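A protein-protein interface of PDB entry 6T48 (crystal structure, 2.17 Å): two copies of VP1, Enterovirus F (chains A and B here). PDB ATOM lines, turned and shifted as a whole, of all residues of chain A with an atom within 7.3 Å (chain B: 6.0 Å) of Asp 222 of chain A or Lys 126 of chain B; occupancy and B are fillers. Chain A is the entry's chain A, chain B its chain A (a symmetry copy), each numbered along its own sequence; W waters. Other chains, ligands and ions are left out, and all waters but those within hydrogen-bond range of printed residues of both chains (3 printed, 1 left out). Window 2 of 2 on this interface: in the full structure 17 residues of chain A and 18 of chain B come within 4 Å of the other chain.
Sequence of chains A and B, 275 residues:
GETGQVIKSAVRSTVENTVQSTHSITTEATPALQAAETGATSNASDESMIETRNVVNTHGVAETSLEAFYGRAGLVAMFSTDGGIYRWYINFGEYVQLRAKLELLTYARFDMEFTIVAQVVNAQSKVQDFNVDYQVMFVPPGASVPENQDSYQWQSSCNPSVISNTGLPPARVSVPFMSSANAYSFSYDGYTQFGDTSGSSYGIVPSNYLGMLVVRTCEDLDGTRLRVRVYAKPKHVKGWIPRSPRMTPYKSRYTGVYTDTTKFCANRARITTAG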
ATOM      1  N   PHE A 130      10.138   8.674 -20.331  1.00  0.00           N
ATOM      2  CA  PHE A 130       9.965   7.837 -21.505  1.00  0.00           C
ATOM      3  C   PHE A 130      10.124   8.701 -22.751  1.00  0.00           C
ATOM      4  O   PHE A 130       9.354   9.631 -22.969  1.00  0.00           O
ATOM      5  CB  PHE A 130       8.560   7.215 -21.437  1.00  0.00           C
ATOM      6  CG  PHE A 130       8.306   6.142 -22.452  1.00  0.00           C
ATOM      7  CD1 PHE A 130       8.087   6.460 -23.787  1.00  0.00           C
ATOM      8  CD2 PHE A 130       8.266   4.808 -22.066  1.00  0.00           C
ATOM      9  CE1 PHE A 130       7.830   5.463 -24.725  1.00  0.00           C
ATOM     10  CE2 PHE A 130       8.008   3.803 -22.996  1.00  0.00           C
ATOM     11  CZ  PHE A 130       7.789   4.131 -24.327  1.00  0.00           C
ATOM     12  N   GLU A 219       4.190   6.300 -33.046  1.00  0.00           N
ATOM     13  CA  GLU A 219       3.761   4.925 -32.810  1.00  0.00           C
ATOM     14  C   GLU A 219       2.924   4.920 -31.532  1.00  0.00           C
ATOM     15  O   GLU A 219       2.988   5.863 -30.746  1.00  0.00           O
ATOM     16  CB  GLU A 219       4.969   3.993 -32.680  1.00  0.00           C
ATOM     17  CG  GLU A 219       5.724   3.758 -33.991  1.00  0.00           C
ATOM     18  CD  GLU A 219       4.850   3.146 -35.085  1.00  0.00           C
ATOM     19  OE1 GLU A 219       4.110   2.182 -34.794  1.00  0.00           O
ATOM     20  OE2 GLU A 219       4.908   3.622 -36.240  1.00  0.00           O
ATOM     21  N   ASP A 220       2.143   3.867 -31.321  1.00  0.00           N
ATOM     22  CA  ASP A 220       1.272   3.796 -30.153  1.00  0.00           C
ATOM     23  C   ASP A 220       1.941   3.589 -28.803  1.00  0.00           C
ATOM     24  O   ASP A 220       2.783   2.710 -28.639  1.00  0.00           O
ATOM     25  CB  ASP A 220       0.218   2.701 -30.342  1.00  0.00           C
ATOM     26  CG  ASP A 220      -0.651   2.930 -31.563  1.00  0.00           C
ATOM     27  OD1 ASP A 220      -1.137   4.066 -31.749  1.00  0.00           O
ATOM     28  OD2 ASP A 220      -0.858   1.968 -32.333  1.00  0.00           O
ATOM     29  N   LEU A 221       1.549   4.416 -27.836  1.00  0.00           N
ATOM     30  CA  LEU A 221       2.049   4.310 -26.473  1.00  0.00           C
ATOM     31  C   LEU A 221       1.194   3.240 -25.804  1.00  0.00           C
ATOM     32  O   LEU A 221       0.041   3.028 -26.185  1.00  0.00           O
ATOM     33  CB  LEU A 221       1.874   5.635 -25.728  1.00  0.00           C
ATOM     34  CG  LEU A 221       2.882   6.743 -26.021  1.00  0.00           C
ATOM     35  CD1 LEU A 221       2.415   8.043 -25.385  1.00  0.00           C
ATOM     36  CD2 LEU A 221       4.244   6.335 -25.474  1.00  0.00           C
ATOM     37  N   ASP A 222       1.749   2.567 -24.807  1.00  0.00           N
ATOM     38  CA  ASP A 222       1.005   1.520 -24.126  1.00  0.00           C
ATOM     39  C   ASP A 222       0.487   1.998 -22.770  1.00  0.00           C
ATOM     40  O   ASP A 222       1.214   1.997 -21.777  1.00  0.00           O
ATOM     41  CB  ASP A 222       1.898   0.280 -23.975  1.00  0.00           C
ATOM     42  CG  ASP A 222       1.125  -0.953 -23.540  1.00  0.00           C
ATOM     43  OD1 ASP A 222      -0.079  -1.053 -23.860  1.00  0.00           O
ATOM     44  OD2 ASP A 222       1.732  -1.831 -22.893  1.00  0.00           O
ATOM     45  N   GLY A 223      -0.772   2.426 -22.748  1.00  0.00           N
ATOM     46  CA  GLY A 223      -1.385   2.891 -21.515  1.00  0.00           C
ATOM     47  C   GLY A 223      -1.066   4.316 -21.097  1.00  0.00           C
ATOM     48  O   GLY A 223      -1.654   4.833 -20.147  1.00  0.00           O
ATOM     49  N   THR A 224      -0.139   4.958 -21.794  1.00  0.00           N
ATOM     50  CA  THR A 224       0.235   6.326 -21.462  1.00  0.00           C
ATOM     51  C   THR A 224      -0.196   7.310 -22.543  1.00  0.00           C
ATOM     52  O   THR A 224      -0.649   6.908 -23.614  1.00  0.00           O
ATOM     53  CB  THR A 224       1.747   6.433 -21.251  1.00  0.00           C
ATOM     54  OG1 THR A 224       2.423   5.884 -22.388  1.00  0.00           O
ATOM     55  CG2 THR A 224       2.163   5.665 -20.001  1.00  0.00           C
ATOM     56  N   ARG A 225      -0.051   8.601 -22.254  1.00  0.00           N
ATOM     57  CA  ARG A 225      -0.437   9.660 -23.184  1.00  0.00           C
ATOM     58  C   ARG A 225       0.676  10.679 -23.340  1.00  0.00           C
ATOM     59  O   ARG A 225       1.605  10.727 -22.535  1.00  0.00           O
ATOM     60  CB  ARG A 225      -1.659  10.415 -22.660  1.00  0.00           C
ATOM     61  CG  ARG A 225      -2.923   9.617 -22.526  1.00  0.00           C
ATOM     62  CD  ARG A 225      -3.927  10.443 -21.754  1.00  0.00           C
ATOM     63  NE  ARG A 225      -3.448  10.694 -20.399  1.00  0.00           N
ATOM     64  CZ  ARG A 225      -4.004  11.554 -19.553  1.00  0.00           C
ATOM     65  NH1 ARG A 225      -5.065  12.259 -19.925  1.00  0.00           N
ATOM     66  NH2 ARG A 225      -3.507  11.697 -18.330  1.00  0.00           N
ATOM     67  N   VAL B 120      11.601   1.504 -31.902  1.00  0.00           N
ATOM     68  CA  VAL B 120      11.441   0.091 -31.597  1.00  0.00           C
ATOM     69  C   VAL B 120      10.007  -0.123 -31.118  1.00  0.00           C
ATOM     70  O   VAL B 120       9.489   0.663 -30.321  1.00  0.00           O
ATOM     71  CB  VAL B 120      12.420  -0.348 -30.486  1.00  0.00           C
ATOM     72  CG1 VAL B 120      12.147  -1.789 -30.080  1.00  0.00           C
ATOM     73  CG2 VAL B 120      13.853  -0.198 -30.978  1.00  0.00           C
ATOM     74  N   VAL B 121       9.357  -1.168 -31.625  1.00  0.00           N
ATOM     75  CA  VAL B 121       7.988  -1.489 -31.222  1.00  0.00           C
ATOM     76  C   VAL B 121       7.933  -2.971 -30.862  1.00  0.00           C
ATOM     77  O   VAL B 121       8.749  -3.754 -31.348  1.00  0.00           O
ATOM     78  CB  VAL B 121       6.968  -1.209 -32.360  1.00  0.00           C
ATOM     79  CG1 VAL B 121       6.975   0.268 -32.718  1.00  0.00           C
ATOM     80  CG2 VAL B 121       7.300  -2.052 -33.584  1.00  0.00           C
ATOM     81  N   ASN B 122       6.991  -3.362 -30.005  1.00  0.00           N
ATOM     82  CA  ASN B 122       6.878  -4.770 -29.633  1.00  0.00           C
ATOM     83  C   ASN B 122       5.905  -5.505 -30.555  1.00  0.00           C
ATOM     84  O   ASN B 122       5.430  -4.946 -31.546  1.00  0.00           O
ATOM     85  CB  ASN B 122       6.442  -4.929 -28.168  1.00  0.00           C
ATOM     86  CG  ASN B 122       5.048  -4.385 -27.897  1.00  0.00           C
ATOM     87  OD1 ASN B 122       4.241  -4.204 -28.810  1.00  0.00           O
ATOM     88  ND2 ASN B 122       4.756  -4.141 -26.625  1.00  0.00           N
ATOM     89  N   ALA B 123       5.613  -6.759 -30.226  1.00  0.00           N
ATOM     90  CA  ALA B 123       4.710  -7.576 -31.035  1.00  0.00           C
ATOM     91  C   ALA B 123       3.303  -6.984 -31.187  1.00  0.00           C
ATOM     92  O   ALA B 123       2.661  -7.161 -32.223  1.00  0.00           O
ATOM     93  CB  ALA B 123       4.628  -8.979 -30.451  1.00  0.00           C
ATOM     94  N   GLN B 124       2.825  -6.292 -30.156  1.00  0.00           N
ATOM     95  CA  GLN B 124       1.498  -5.677 -30.195  1.00  0.00           C
ATOM     96  C   GLN B 124       1.569  -4.288 -30.821  1.00  0.00           C
ATOM     97  O   GLN B 124       0.617  -3.514 -30.747  1.00  0.00           O
ATOM     98  CB  GLN B 124       0.913  -5.565 -28.783  1.00  0.00           C
ATOM     99  CG  GLN B 124       0.612  -6.897 -28.120  1.00  0.00           C
ATOM    100  CD  GLN B 124       1.853  -7.741 -27.922  1.00  0.00           C
ATOM    101  OE1 GLN B 124       2.806  -7.324 -27.261  1.00  0.00           O
ATOM    102  NE2 GLN B 124       1.849  -8.940 -28.494  1.00  0.00           N
ATOM    103  N   SER B 125       2.708  -3.982 -31.432  1.00  0.00           N
ATOM    104  CA  SER B 125       2.927  -2.696 -32.081  1.00  0.00           C
ATOM    105  C   SER B 125       2.894  -1.503 -31.129  1.00  0.00           C
ATOM    106  O   SER B 125       2.457  -0.415 -31.499  1.00  0.00           O
ATOM    107  CB  SER B 125       1.910  -2.493 -33.207  1.00  0.00           C
ATOM    108  OG  SER B 125       2.112  -3.442 -34.237  1.00  0.00           O
ATOM    109  N   LYS B 126       3.347  -1.709 -29.898  1.00  0.00           N
ATOM    110  CA  LYS B 126       3.401  -0.624 -28.927  1.00  0.00           C
ATOM    111  C   LYS B 126       4.843  -0.120 -28.917  1.00  0.00           C
ATOM    112  O   LYS B 126       5.783  -0.910 -28.839  1.00  0.00           O
ATOM    113  CB  LYS B 126       2.993  -1.117 -27.535  1.00  0.00           C
ATOM    114  CG  LYS B 126       1.513  -1.467 -27.413  1.00  0.00           C
ATOM    115  CD  LYS B 126       0.635  -0.268 -27.753  1.00  0.00           C
ATOM    116  CE  LYS B 126      -0.842  -0.550 -27.512  1.00  0.00           C
ATOM    117  NZ  LYS B 126      -1.342  -1.656 -28.368  1.00  0.00           N
ATOM    118  N   VAL B 127       5.011   1.194 -29.010  1.00  0.00           N
ATOM    119  CA  VAL B 127       6.342   1.787 -29.040  1.00  0.00           C
ATOM    120  C   VAL B 127       7.119   1.554 -27.743  1.00  0.00           C
ATOM    121  O   VAL B 127       6.553   1.544 -26.651  1.00  0.00           O
ATOM    122  CB  VAL B 127       6.260   3.305 -29.338  1.00  0.00           C
ATOM    123  CG1 VAL B 127       5.739   4.054 -28.123  1.00  0.00           C
ATOM    124  CG2 VAL B 127       7.622   3.825 -29.767  1.00  0.00           C
ATOM    125  N   GLN B 128       8.425   1.358 -27.880  1.00  0.00           N
ATOM    126  CA  GLN B 128       9.293   1.116 -26.735  1.00  0.00           C
ATOM    127  C   GLN B 128      10.350   2.211 -26.618  1.00  0.00           C
ATOM    128  O   GLN B 128      10.780   2.775 -27.625  1.00  0.00           O
ATOM    129  CB  GLN B 128      10.005  -0.229 -26.902  1.00  0.00           C
ATOM    130  CG  GLN B 128       9.084  -1.403 -27.161  1.00  0.00           C
ATOM    131  CD  GLN B 128       8.238  -1.737 -25.958  1.00  0.00           C
ATOM    132  OE1 GLN B 128       8.760  -2.051 -24.889  1.00  0.00           O
ATOM    133  NE2 GLN B 128       6.921  -1.671 -26.122  1.00  0.00           N
HETATM  134  O   HOH W   1       4.500   2.226 -24.519  1.00  0.00           O
HETATM  135  O   HOH W   2       2.103   1.645 -33.185  1.00  0.00           O
HETATM  136  O   HOH W   3       4.883  -1.688 -24.003  1.00  0.00           O
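O of Asp 220 of chain A is in hydrogen-bond range of N of Val 127 of chain B, at 2.7 Å.
The backbone carbonyl oxygen of Val 120 of chain B sits at hydrogen-bond distance from the backbone NH of Gln 128 of chain B (2.8 Å). The side-chain amide oxygen (OD1) of Asn 122 of chain B lies within hydrogen-bond range of the backbone NH (N) of Lys 126 of chain B. NE2 of Gln 128 of chain B lies close to ND2 of Asn 122 of chain B (3.3 Å). The backbone carbonyl oxygen (O) of Lys 126 of chain B is in hydrogen-bond range of the side-chain amide nitrogen (NE2) of Gln 128 of chain B, 3.0 Å away.
Phe 130 of chain A touches Val 127 of chain B (CZ to O, 3.7 Å). Phe 130 of chain A touches Gln 128 of chain B (CZ to C, 3.9 Å). Glu 219 of chain A touches Val 121 of chain B. Glu 219 of chain A touches Val 127 of chain B (CB to CB, 3.6 Å). O of Asp 220 of chain A touches CA of Lys 126 of chain B, 3.4 Å away. Lys 126 of chain B touches Leu 221 of chain A (CD to O, 3.7 Å). Leu 221 of chain A touches Val 127 of chain B. Asp 222 of chain A touches Lys 126 of chain B (OD1 to CE, 3.8 Å).
Printed residues of chain B within 4 Å of Phe 130 of chain A: Val 127 (3.7 Å) and Gln 128 (3.9 Å). Of the printed residues of chain B, Leu 221 of chain A touches Lys 126 (3.7 Å) and Val 127 (3.8 Å). Arg 225 of chain A touches none of the printed residues of chain B. Val 120 of chain B touches none of the printed residues of chain A. Of chain A, only Asp 220 (3.4 Å), Leu 221 (3.7 Å) and Asp 222 (3.8 Å) come within 4 Å of Lys 126 of chain B. Of the printed residues of chain A, Gln 128 of chain B touches Phe 130 (3.9 Å). The nearest residue of chain B that does not touch Asp 222 of chain A is Val 127 of chain B (5.2 Å). The nearest residue of chain A that does not touch Lys 126 of chain B is Glu 219 of chain A (5.6 Å).
Printed residues of chain A that touch a printed residue of chain B: Phe 130, Glu 219, Asp 220, Leu 221 and Asp 222. Hydrophobic or aromatic side chains of chain A within 4 Å of the printed part of chain B: Phe 130 and Leu 221. Printed residues of chain B that touch a printed residue of chain A: Val 121, Lys 126, Val 127 and Gln 128. Among the printed residues, 9 pairs touch across the chains. Among the printed residues, no Asp or Glu carboxylate lies within 4 Å of a Lys or Arg side-chain nitrogen of the other chain.
No position is printed for both chains. Of the 9 pairs that touch across the chains among the printed residues, none has its exchanged pair printed and touching as well.
Water W2 lies within hydrogen-bond range of OE1 of Glu 219 of chain A (2.6 Å), O of Ser 125 of chain B (2.7 Å) and N of Asp 220 of chain A (2.9 Å). Water W1 bridges the backbone NH of Asp 222 of chain A and the backbone carbonyl oxygen of Val 127 of chain B. Water W3 bridges NE2 of Gln 128 of chain B (2.9 Å) and OD2 of Asp 222 of chain A (3.3 Å).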
